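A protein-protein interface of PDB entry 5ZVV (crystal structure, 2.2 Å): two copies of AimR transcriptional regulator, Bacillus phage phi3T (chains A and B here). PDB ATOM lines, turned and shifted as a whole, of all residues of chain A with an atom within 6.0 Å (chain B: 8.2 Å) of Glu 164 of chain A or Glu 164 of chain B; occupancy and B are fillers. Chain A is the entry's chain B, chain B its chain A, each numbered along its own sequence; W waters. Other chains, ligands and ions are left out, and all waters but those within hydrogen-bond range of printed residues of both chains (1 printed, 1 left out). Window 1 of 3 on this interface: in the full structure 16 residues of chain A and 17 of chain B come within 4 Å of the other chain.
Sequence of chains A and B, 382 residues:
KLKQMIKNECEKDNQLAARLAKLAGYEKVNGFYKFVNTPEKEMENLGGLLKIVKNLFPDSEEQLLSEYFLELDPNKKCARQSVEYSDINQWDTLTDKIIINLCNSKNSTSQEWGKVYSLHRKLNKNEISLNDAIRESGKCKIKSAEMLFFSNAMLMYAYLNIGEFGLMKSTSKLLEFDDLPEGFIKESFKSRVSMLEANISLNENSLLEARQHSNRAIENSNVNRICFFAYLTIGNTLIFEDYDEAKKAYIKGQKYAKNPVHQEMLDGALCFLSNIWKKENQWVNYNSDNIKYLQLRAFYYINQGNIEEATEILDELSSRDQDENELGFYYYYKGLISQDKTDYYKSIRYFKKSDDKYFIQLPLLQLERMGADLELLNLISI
The backbone NH (N) of Leu 167 of chain B lies within hydrogen-bond range of the side-chain carboxylate (OE2) of Glu 164 of chain A (3.4 Å).
O of Leu 167 of chain B is in hydrogen-bond range of OG of Ser 170 of chain B (3.3 Å). The backbone carbonyl oxygen (O) of Leu 167 of chain B sits at hydrogen-bond distance from the side-chain hydroxyl (OG1) of Thr 171 of chain B, 2.6 Å away. The side-chain hydroxyl of Ser 170 of chain B sits at hydrogen-bond distance from the backbone carbonyl oxygen of Gly 166 of chain B. The backbone carbonyl oxygen of Tyr 159 of chain A is in hydrogen-bond range of the backbone NH of Glu 164 of chain A. The backbone carbonyl oxygen of Tyr 159 of chain B lies within hydrogen-bond range of the backbone NH of Glu 164 of chain B.
Among the printed residues, merely in contact across the chains: Glu 164 of chain A with Gly 166 of chain B (3.4 Å), Gly 166 of chain A with Glu 164 of chain B (3.4 Å), Leu 167 of chain A with Leu 167 of chain B (3.6 Å), Leu 167 of chain A with Glu 164 of chain B (3.7 Å) and Glu 164 of chain A with Glu 164 of chain B (3.8 Å).
Glu 164 of chain A touches just these residues of chain B: Glu 164, Gly 166 and Leu 167. Of chain A, only Glu 164 (3.8 Å), Gly 166 (3.4 Å) and Leu 167 (3.7 Å) come within 4 Å of Glu 164 of chain B. No residue of chain B comes within 4 Å of Gly 163 of chain A. Of the printed residues of chain A, Leu 167 of chain B touches Glu 164 and Leu 167. Of the printed residues of chain B, Gly 166 of chain A touches Glu 164. Of the printed residues of chain B, Leu 167 of chain A touches Glu 164 (3.7 Å) and Leu 167 (3.6 Å). Met 156 of chain B touches none of the printed residues of chain A. The nearest residue of chain B that does not touch Glu 164 of chain A is Ser 170 of chain B (5.2 Å). The nearest printed residue of chain B that does not touch Leu 167 of chain A is Ile 162 of chain B (4.7 Å).
Printed residues of chain B that touch a printed residue of chain A: Glu 164, Gly 166 and Leu 167. Hydrophobic or aromatic side chains of chain B that line the printed part of chain A: Leu 167. Hydrophobic or aromatic side chains of chain A that line the printed part of chain B: Leu 167.
Glu 164 of chain B touches its own counterpart, Glu 164 of chain A. Glu 164 of chain A touches Gly 166 of chain B, and with the chains exchanged Gly 166 of chain A touches Glu 164 of chain B. Glu 164 of chain A touches Leu 167 of chain B, and with the chains exchanged Leu 167 of chain A touches Glu 164 of chain B. Leu 167 of chain A touches its own counterpart, Leu 167 of chain B. 11 positions are printed for both chains. Of the 6 pairs that touch across the chains among the printed residues, 6 have their exchanged pair printed and touching as well.
Water W1 lies within hydrogen-bond range of the side-chain carboxylate (OE1) of Glu 164 of chain A (2.6 Å), the backbone NH (N) of Leu 167 of chain B (2.7 Å), the side-chain carboxylate (OE1) of Glu 164 of chain B (2.8 Å) and the backbone NH (N) of Gly 166 of chain B (3.2 Å).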
ATOM      1  N   TYR A 159      20.140 -12.572 -11.672  1.00  0.00           N
ATOM      2  CA  TYR A 159      21.318 -12.609 -10.810  1.00  0.00           C
ATOM      3  C   TYR A 159      22.102 -11.306 -10.880  1.00  0.00           C
ATOM      4  O   TYR A 159      22.701 -10.888  -9.882  1.00  0.00           O
ATOM      5  CB  TYR A 159      22.208 -13.792 -11.192  1.00  0.00           C
ATOM      6  CG  TYR A 159      21.693 -15.133 -10.726  1.00  0.00           C
ATOM      7  CD1 TYR A 159      21.308 -15.330  -9.405  1.00  0.00           C
ATOM      8  CD2 TYR A 159      21.587 -16.203 -11.605  1.00  0.00           C
ATOM      9  CE1 TYR A 159      20.838 -16.559  -8.972  1.00  0.00           C
ATOM     10  CE2 TYR A 159      21.113 -17.434 -11.183  1.00  0.00           C
ATOM     11  CZ  TYR A 159      20.740 -17.606  -9.867  1.00  0.00           C
ATOM     12  OH  TYR A 159      20.272 -18.827  -9.444  1.00  0.00           O
ATOM     13  N   LEU A 160      22.112 -10.651 -12.043  1.00  0.00           N
ATOM     14  CA  LEU A 160      22.784  -9.359 -12.153  1.00  0.00           C
ATOM     15  C   LEU A 160      22.082  -8.298 -11.317  1.00  0.00           C
ATOM     16  O   LEU A 160      22.739  -7.447 -10.704  1.00  0.00           O
ATOM     17  CB  LEU A 160      22.854  -8.927 -13.617  1.00  0.00           C
ATOM     18  CG  LEU A 160      23.449  -7.543 -13.901  1.00  0.00           C
ATOM     19  CD1 LEU A 160      24.896  -7.467 -13.443  1.00  0.00           C
ATOM     20  CD2 LEU A 160      23.335  -7.200 -15.380  1.00  0.00           C
ATOM     21  N   ASN A 161      20.747  -8.335 -11.273  1.00  0.00           N
ATOM     22  CA  ASN A 161      20.000  -7.321 -10.535  1.00  0.00           C
ATOM     23  C   ASN A 161      20.252  -7.408  -9.036  1.00  0.00           C
ATOM     24  O   ASN A 161      20.133  -6.399  -8.332  1.00  0.00           O
ATOM     25  CB  ASN A 161      18.507  -7.447 -10.830  1.00  0.00           C
ATOM     26  CG  ASN A 161      18.133  -6.893 -12.190  1.00  0.00           C
ATOM     27  OD1 ASN A 161      18.666  -5.871 -12.622  1.00  0.00           O
ATOM     28  ND2 ASN A 161      17.214  -7.567 -12.873  1.00  0.00           N
ATOM     29  N   ILE A 162      20.596  -8.592  -8.528  1.00  0.00           N
ATOM     30  CA  ILE A 162      20.912  -8.759  -7.116  1.00  0.00           C
ATOM     31  C   ILE A 162      22.415  -8.847  -6.876  1.00  0.00           C
ATOM     32  O   ILE A 162      22.842  -9.210  -5.777  1.00  0.00           O
ATOM     33  CB  ILE A 162      20.190  -9.979  -6.525  1.00  0.00           C
ATOM     34  CG1 ILE A 162      20.578 -11.254  -7.275  1.00  0.00           C
ATOM     35  CG2 ILE A 162      18.682  -9.771  -6.559  1.00  0.00           C
ATOM     36  CD1 ILE A 162      19.901 -12.498  -6.743  1.00  0.00           C
ATOM     37  N   GLY A 163      23.227  -8.525  -7.880  1.00  0.00           N
ATOM     38  CA  GLY A 163      24.670  -8.500  -7.709  1.00  0.00           C
ATOM     39  C   GLY A 163      25.305  -9.842  -7.412  1.00  0.00           C
ATOM     40  O   GLY A 163      26.374  -9.889  -6.794  1.00  0.00           O
ATOM     41  N   GLU A 164      24.680 -10.940  -7.837  1.00  0.00           N
ATOM     42  CA  GLU A 164      25.227 -12.278  -7.607  1.00  0.00           C
ATOM     43  C   GLU A 164      25.968 -12.717  -8.867  1.00  0.00           C
ATOM     44  O   GLU A 164      25.452 -13.449  -9.710  1.00  0.00           O
ATOM     45  CB  GLU A 164      24.123 -13.257  -7.217  1.00  0.00           C
ATOM     46  CG  GLU A 164      23.496 -12.977  -5.854  1.00  0.00           C
ATOM     47  CD  GLU A 164      24.461 -13.184  -4.698  1.00  0.00           C
ATOM     48  OE1 GLU A 164      25.546 -13.765  -4.911  1.00  0.00           O
ATOM     49  OE2 GLU A 164      24.132 -12.767  -3.568  1.00  0.00           O
ATOM     50  N   PHE A 165      27.214 -12.253  -8.980  1.00  0.00           N
ATOM     51  CA  PHE A 165      27.990 -12.491 -10.193  1.00  0.00           C
ATOM     52  C   PHE A 165      28.503 -13.921 -10.268  1.00  0.00           C
ATOM     53  O   PHE A 165      28.737 -14.434 -11.369  1.00  0.00           O
ATOM     54  CB  PHE A 165      29.148 -11.496 -10.274  1.00  0.00           C
ATOM     55  CG  PHE A 165      28.704 -10.067 -10.381  1.00  0.00           C
ATOM     56  CD1 PHE A 165      28.465  -9.492 -11.619  1.00  0.00           C
ATOM     57  CD2 PHE A 165      28.512  -9.298  -9.242  1.00  0.00           C
ATOM     58  CE1 PHE A 165      28.048  -8.176 -11.721  1.00  0.00           C
ATOM     59  CE2 PHE A 165      28.094  -7.981  -9.338  1.00  0.00           C
ATOM     60  CZ  PHE A 165      27.861  -7.421 -10.578  1.00  0.00           C
ATOM     61  N   GLY A 166      28.686 -14.578  -9.124  1.00  0.00           N
ATOM     62  CA  GLY A 166      29.109 -15.965  -9.129  1.00  0.00           C
ATOM     63  C   GLY A 166      28.108 -16.846  -9.848  1.00  0.00           C
ATOM     64  O   GLY A 166      28.453 -17.535 -10.816  1.00  0.00           O
ATOM     65  N   LEU A 167      26.852 -16.802  -9.397  1.00  0.00           N
ATOM     66  CA  LEU A 167      25.810 -17.607 -10.029  1.00  0.00           C
ATOM     67  C   LEU A 167      25.672 -17.271 -11.509  1.00  0.00           C
ATOM     68  O   LEU A 167      25.546 -18.178 -12.343  1.00  0.00           O
ATOM     69  CB  LEU A 167      24.482 -17.418  -9.298  1.00  0.00           C
ATOM     70  CG  LEU A 167      24.137 -18.547  -8.321  1.00  0.00           C
ATOM     71  CD1 LEU A 167      23.706 -19.798  -9.073  1.00  0.00           C
ATOM     72  CD2 LEU A 167      25.326 -18.854  -7.419  1.00  0.00           C
ATOM     73  N   MET A 168      25.711 -15.981 -11.852  1.00  0.00           N
ATOM     74  CA  MET A 168      25.784 -15.543 -13.247  1.00  0.00           C
ATOM     75  C   MET A 168      26.769 -16.419 -13.996  1.00  0.00           C
ATOM     76  O   MET A 168      26.394 -17.118 -14.945  1.00  0.00           O
ATOM     77  CB  MET A 168      26.218 -14.073 -13.362  1.00  0.00           C
ATOM     78  CG  MET A 168      25.179 -13.044 -12.942  1.00  0.00           C
ATOM     79  SD  MET A 168      25.702 -11.198 -13.354  1.00  0.00           S
ATOM     80  CE  MET A 168      25.608 -11.270 -15.306  1.00  0.00           C
ATOM     81  N   LYS A 169      28.018 -16.406 -13.518  1.00  0.00           N
ATOM     82  CA  LYS A 169      29.065 -17.213 -14.137  1.00  0.00           C
ATOM     83  C   LYS A 169      28.614 -18.659 -14.290  1.00  0.00           C
ATOM     84  O   LYS A 169      28.602 -19.204 -15.401  1.00  0.00           O
ATOM     85  CB  LYS A 169      30.351 -17.129 -13.313  1.00  0.00           C
ATOM     86  CG  LYS A 169      30.949 -15.732 -13.237  1.00  0.00           C
ATOM     87  CD  LYS A 169      32.192 -15.692 -12.354  1.00  0.00           C
ATOM     88  CE  LYS A 169      33.341 -16.482 -12.967  1.00  0.00           C
ATOM     89  NZ  LYS A 169      34.573 -16.428 -12.125  1.00  0.00           N
ATOM     90  N   LEU B 130      21.900 -27.575  -7.741  1.00  0.00           N
ATOM     91  CA  LEU B 130      21.179 -26.664  -6.859  1.00  0.00           C
ATOM     92  C   LEU B 130      19.883 -26.191  -7.508  1.00  0.00           C
ATOM     93  O   LEU B 130      18.820 -26.184  -6.873  1.00  0.00           O
ATOM     94  CB  LEU B 130      22.075 -25.481  -6.495  1.00  0.00           C
ATOM     95  CG  LEU B 130      21.604 -24.555  -5.378  1.00  0.00           C
ATOM     96  CD1 LEU B 130      22.791 -24.122  -4.537  1.00  0.00           C
ATOM     97  CD2 LEU B 130      20.889 -23.341  -5.951  1.00  0.00           C
ATOM     98  N   LEU B 155      19.022 -24.901   1.384  1.00  0.00           N
ATOM     99  CA  LEU B 155      19.785 -24.279   0.310  1.00  0.00           C
ATOM    100  C   LEU B 155      21.016 -23.568   0.851  1.00  0.00           C
ATOM    101  O   LEU B 155      22.003 -23.403   0.128  1.00  0.00           O
ATOM    102  CB  LEU B 155      18.903 -23.298  -0.465  1.00  0.00           C
ATOM    103  CG  LEU B 155      17.715 -23.881  -1.226  1.00  0.00           C
ATOM    104  CD1 LEU B 155      16.990 -22.790  -2.001  1.00  0.00           C
ATOM    105  CD2 LEU B 155      18.159 -25.000  -2.165  1.00  0.00           C
ATOM    106  N   MET B 156      20.981 -23.154   2.114  1.00  0.00           N
ATOM    107  CA  MET B 156      22.091 -22.430   2.728  1.00  0.00           C
ATOM    108  C   MET B 156      23.328 -23.303   2.877  1.00  0.00           C
ATOM    109  O   MET B 156      24.452 -22.810   2.773  1.00  0.00           O
ATOM    110  CB  MET B 156      21.677 -21.880   4.094  1.00  0.00           C
ATOM    111  CG  MET B 156      20.558 -20.863   4.035  1.00  0.00           C
ATOM    112  SD  MET B 156      20.087 -20.189   5.801  1.00  0.00           S
ATOM    113  CE  MET B 156      21.742 -19.235   6.216  1.00  0.00           C
ATOM    114  N   TYR B 157      23.121 -24.599   3.129  1.00  0.00           N
ATOM    115  CA  TYR B 157      24.254 -25.514   3.217  1.00  0.00           C
ATOM    116  C   TYR B 157      24.956 -25.644   1.872  1.00  0.00           C
ATOM    117  O   TYR B 157      26.191 -25.621   1.806  1.00  0.00           O
ATOM    118  CB  TYR B 157      23.798 -26.883   3.722  1.00  0.00           C
ATOM    119  CG  TYR B 157      23.304 -26.875   5.153  1.00  0.00           C
ATOM    120  CD1 TYR B 157      24.190 -26.737   6.212  1.00  0.00           C
ATOM    121  CD2 TYR B 157      21.953 -27.013   5.443  1.00  0.00           C
ATOM    122  CE1 TYR B 157      23.742 -26.728   7.521  1.00  0.00           C
ATOM    123  CE2 TYR B 157      21.496 -27.006   6.746  1.00  0.00           C
ATOM    124  CZ  TYR B 157      22.397 -26.863   7.782  1.00  0.00           C
ATOM    125  OH  TYR B 157      21.947 -26.858   9.081  1.00  0.00           O
ATOM    126  N   ALA B 158      24.188 -25.782   0.789  1.00  0.00           N
ATOM    127  CA  ALA B 158      24.787 -25.876  -0.538  1.00  0.00           C
ATOM    128  C   ALA B 158      25.505 -24.583  -0.910  1.00  0.00           C
ATOM    129  O   ALA B 158      26.642 -24.611  -1.402  1.00  0.00           O
ATOM    130  CB  ALA B 158      23.715 -26.218  -1.573  1.00  0.00           C
ATOM    131  N   TYR B 159      24.853 -23.436  -0.677  1.00  0.00           N
ATOM    132  CA  TYR B 159      25.494 -22.148  -0.926  1.00  0.00           C
ATOM    133  C   TYR B 159      26.772 -22.003  -0.110  1.00  0.00           C
ATOM    134  O   TYR B 159      27.770 -21.460  -0.597  1.00  0.00           O
ATOM    135  CB  TYR B 159      24.529 -21.006  -0.610  1.00  0.00           C
ATOM    136  CG  TYR B 159      23.422 -20.821  -1.621  1.00  0.00           C
ATOM    137  CD1 TYR B 159      23.690 -20.824  -2.983  1.00  0.00           C
ATOM    138  CD2 TYR B 159      22.106 -20.643  -1.213  1.00  0.00           C
ATOM    139  CE1 TYR B 159      22.679 -20.654  -3.909  1.00  0.00           C
ATOM    140  CE2 TYR B 159      21.089 -20.478  -2.131  1.00  0.00           C
ATOM    141  CZ  TYR B 159      21.381 -20.484  -3.479  1.00  0.00           C
ATOM    142  OH  TYR B 159      20.371 -20.316  -4.397  1.00  0.00           O
ATOM    143  N   LEU B 160      26.753 -22.473   1.141  1.00  0.00           N
ATOM    144  CA  LEU B 160      27.979 -22.524   1.928  1.00  0.00           C
ATOM    145  C   LEU B 160      29.003 -23.446   1.283  1.00  0.00           C
ATOM    146  O   LEU B 160      30.201 -23.139   1.259  1.00  0.00           O
ATOM    147  CB  LEU B 160      27.674 -22.989   3.352  1.00  0.00           C
ATOM    148  CG  LEU B 160      28.882 -23.302   4.236  1.00  0.00           C
ATOM    149  CD1 LEU B 160      29.674 -22.040   4.531  1.00  0.00           C
ATOM    150  CD2 LEU B 160      28.446 -23.988   5.523  1.00  0.00           C
ATOM    151  N   ASN B 161      28.549 -24.580   0.744  1.00  0.00           N
ATOM    152  CA  ASN B 161      29.476 -25.527   0.139  1.00  0.00           C
ATOM    153  C   ASN B 161      30.163 -24.937  -1.085  1.00  0.00           C
ATOM    154  O   ASN B 161      31.298 -25.310  -1.396  1.00  0.00           O
ATOM    155  CB  ASN B 161      28.747 -26.821  -0.226  1.00  0.00           C
ATOM    156  CG  ASN B 161      29.695 -27.913  -0.683  1.00  0.00           C
ATOM    157  OD1 ASN B 161      30.438 -28.479   0.119  1.00  0.00           O
ATOM    158  ND2 ASN B 161      29.669 -28.221  -1.976  1.00  0.00           N
ATOM    159  N   ILE B 162      29.504 -24.015  -1.788  1.00  0.00           N
ATOM    160  CA  ILE B 162      30.117 -23.344  -2.931  1.00  0.00           C
ATOM    161  C   ILE B 162      30.563 -21.925  -2.592  1.00  0.00           C
ATOM    162  O   ILE B 162      30.888 -21.148  -3.496  1.00  0.00           O
ATOM    163  CB  ILE B 162      29.181 -23.348  -4.150  1.00  0.00           C
ATOM    164  CG1 ILE B 162      27.853 -22.670  -3.815  1.00  0.00           C
ATOM    165  CG2 ILE B 162      28.953 -24.774  -4.640  1.00  0.00           C
ATOM    166  CD1 ILE B 162      26.897 -22.591  -4.994  1.00  0.00           C
ATOM    167  N   GLY B 163      30.589 -21.568  -1.310  1.00  0.00           N
ATOM    168  CA  GLY B 163      31.109 -20.276  -0.893  1.00  0.00           C
ATOM    169  C   GLY B 163      30.318 -19.083  -1.383  1.00  0.00           C
ATOM    170  O   GLY B 163      30.882 -17.994  -1.532  1.00  0.00           O
ATOM    171  N   GLU B 164      29.022 -19.255  -1.640  1.00  0.00           N
ATOM    172  CA  GLU B 164      28.168 -18.164  -2.107  1.00  0.00           C
ATOM    173  C   GLU B 164      27.469 -17.553  -0.896  1.00  0.00           C
ATOM    174  O   GLU B 164      26.282 -17.764  -0.648  1.00  0.00           O
ATOM    175  CB  GLU B 164      27.178 -18.665  -3.152  1.00  0.00           C
ATOM    176  CG  GLU B 164      27.809 -19.036  -4.488  1.00  0.00           C
ATOM    177  CD  GLU B 164      28.224 -17.825  -5.307  1.00  0.00           C
ATOM    178  OE1 GLU B 164      27.948 -16.683  -4.883  1.00  0.00           O
ATOM    179  OE2 GLU B 164      28.825 -18.017  -6.385  1.00  0.00           O
ATOM    180  N   PHE B 165      28.236 -16.768  -0.135  1.00  0.00           N
ATOM    181  CA  PHE B 165      27.744 -16.250   1.139  1.00  0.00           C
ATOM    182  C   PHE B 165      26.573 -15.296   0.941  1.00  0.00           C
ATOM    183  O   PHE B 165      25.611 -15.323   1.717  1.00  0.00           O
ATOM    184  CB  PHE B 165      28.880 -15.566   1.899  1.00  0.00           C
ATOM    185  CG  PHE B 165      30.007 -16.492   2.257  1.00  0.00           C
ATOM    186  CD1 PHE B 165      29.912 -17.321   3.361  1.00  0.00           C
ATOM    187  CD2 PHE B 165      31.157 -16.538   1.487  1.00  0.00           C
ATOM    188  CE1 PHE B 165      30.946 -18.180   3.694  1.00  0.00           C
ATOM    189  CE2 PHE B 165      32.196 -17.392   1.811  1.00  0.00           C
ATOM    190  CZ  PHE B 165      32.090 -18.216   2.916  1.00  0.00           C
ATOM    191  N   GLY B 166      26.633 -14.449  -0.090  1.00  0.00           N
ATOM    192  CA  GLY B 166      25.517 -13.555  -0.363  1.00  0.00           C
ATOM    193  C   GLY B 166      24.205 -14.299  -0.498  1.00  0.00           C
ATOM    194  O   GLY B 166      23.214 -13.970   0.160  1.00  0.00           O
ATOM    195  N   LEU B 167      24.192 -15.344  -1.331  1.00  0.00           N
ATOM    196  CA  LEU B 167      22.982 -16.137  -1.499  1.00  0.00           C
ATOM    197  C   LEU B 167      22.612 -16.907  -0.242  1.00  0.00           C
ATOM    198  O   LEU B 167      21.456 -17.317  -0.104  1.00  0.00           O
ATOM    199  CB  LEU B 167      23.137 -17.096  -2.676  1.00  0.00           C
ATOM    200  CG  LEU B 167      22.569 -16.501  -3.962  1.00  0.00           C
ATOM    201  CD1 LEU B 167      23.113 -17.228  -5.160  1.00  0.00           C
ATOM    202  CD2 LEU B 167      21.051 -16.568  -3.943  1.00  0.00           C
ATOM    203  N   MET B 168      23.554 -17.119   0.671  1.00  0.00           N
ATOM    204  CA  MET B 168      23.190 -17.636   1.979  1.00  0.00           C
ATOM    205  C   MET B 168      22.344 -16.578   2.664  1.00  0.00           C
ATOM    206  O   MET B 168      21.202 -16.835   3.064  1.00  0.00           O
ATOM    207  CB  MET B 168      24.422 -17.968   2.830  1.00  0.00           C
ATOM    208  CG  MET B 168      25.234 -19.155   2.346  1.00  0.00           C
ATOM    209  SD  MET B 168      26.736 -19.586   3.524  1.00  0.00           S
ATOM    210  CE  MET B 168      25.728 -20.204   5.083  1.00  0.00           C
ATOM    211  N   LYS B 169      22.909 -15.369   2.753  1.00  0.00           N
ATOM    212  CA  LYS B 169      22.273 -14.304   3.522  1.00  0.00           C
ATOM    213  C   LYS B 169      20.862 -14.037   3.017  1.00  0.00           C
ATOM    214  O   LYS B 169      19.894 -14.097   3.787  1.00  0.00           O
ATOM    215  CB  LYS B 169      23.132 -13.041   3.466  1.00  0.00           C
ATOM    216  CG  LYS B 169      24.536 -13.254   4.022  1.00  0.00           C
ATOM    217  CD  LYS B 169      25.423 -12.033   3.836  1.00  0.00           C
ATOM    218  CE  LYS B 169      24.969 -10.875   4.708  1.00  0.00           C
ATOM    219  NZ  LYS B 169      25.881  -9.705   4.573  1.00  0.00           N
ATOM    220  N   SER B 170      20.723 -13.792   1.711  1.00  0.00           N
ATOM    221  CA  SER B 170      19.402 -13.560   1.137  1.00  0.00           C
ATOM    222  C   SER B 170      18.455 -14.709   1.456  1.00  0.00           C
ATOM    223  O   SER B 170      17.297 -14.479   1.828  1.00  0.00           O
ATOM    224  CB  SER B 170      19.511 -13.346  -0.374  1.00  0.00           C
ATOM    225  OG  SER B 170      19.998 -14.503  -1.034  1.00  0.00           O
ATOM    226  N   THR B 171      18.938 -15.954   1.356  1.00  0.00           N
ATOM    227  CA  THR B 171      18.079 -17.089   1.677  1.00  0.00           C
ATOM    228  C   THR B 171      17.567 -16.991   3.108  1.00  0.00           C
ATOM    229  O   THR B 171      16.369 -17.165   3.361  1.00  0.00           O
ATOM    230  CB  THR B 171      18.825 -18.409   1.464  1.00  0.00           C
ATOM    231  OG1 THR B 171      19.154 -18.558   0.077  1.00  0.00           O
ATOM    232  CG2 THR B 171      17.955 -19.586   1.889  1.00  0.00           C
ATOM    233  N   ILE B 200      28.646 -17.314   8.807  1.00  0.00           N
ATOM    234  CA  ILE B 200      28.558 -16.134   7.947  1.00  0.00           C
ATOM    235  C   ILE B 200      29.210 -14.936   8.625  1.00  0.00           C
ATOM    236  O   ILE B 200      30.019 -14.218   8.022  1.00  0.00           O
ATOM    237  CB  ILE B 200      27.094 -15.832   7.585  1.00  0.00           C
ATOM    238  CG1 ILE B 200      26.519 -16.916   6.673  1.00  0.00           C
ATOM    239  CG2 ILE B 200      26.984 -14.467   6.925  1.00  0.00           C
ATOM    240  CD1 ILE B 200      25.058 -16.706   6.344  1.00  0.00           C
ATOM    241  N   ASN B 203      32.996 -15.175   8.886  1.00  0.00           N
ATOM    242  CA  ASN B 203      33.661 -14.979   7.603  1.00  0.00           C
ATOM    243  C   ASN B 203      33.781 -13.502   7.251  1.00  0.00           C
ATOM    244  O   ASN B 203      34.737 -13.102   6.574  1.00  0.00           O
ATOM    245  CB  ASN B 203      32.913 -15.730   6.503  1.00  0.00           C
ATOM    246  CG  ASN B 203      33.672 -15.744   5.191  1.00  0.00           C
ATOM    247  OD1 ASN B 203      34.688 -16.427   5.059  1.00  0.00           O
ATOM    248  ND2 ASN B 203      33.179 -14.996   4.211  1.00  0.00           N
ATOM    249  N   ASP B 355      37.213 -14.674  -0.345  1.00  0.00           N
ATOM    250  CA  ASP B 355      36.288 -13.829   0.413  1.00  0.00           C
ATOM    251  C   ASP B 355      36.453 -14.045   1.917  1.00  0.00           C
ATOM    252  O   ASP B 355      35.479 -14.067   2.674  1.00  0.00           O
ATOM    253  CB  ASP B 355      34.840 -14.072  -0.024  1.00  0.00           C
ATOM    254  CG  ASP B 355      33.908 -12.943   0.373  1.00  0.00           C
ATOM    255  OD1 ASP B 355      34.397 -11.902   0.859  1.00  0.00           O
ATOM    256  OD2 ASP B 355      32.680 -13.101   0.194  1.00  0.00           O
HETATM  257  O   HOH W   1      26.274 -15.409  -3.080  1.00  0.00           O
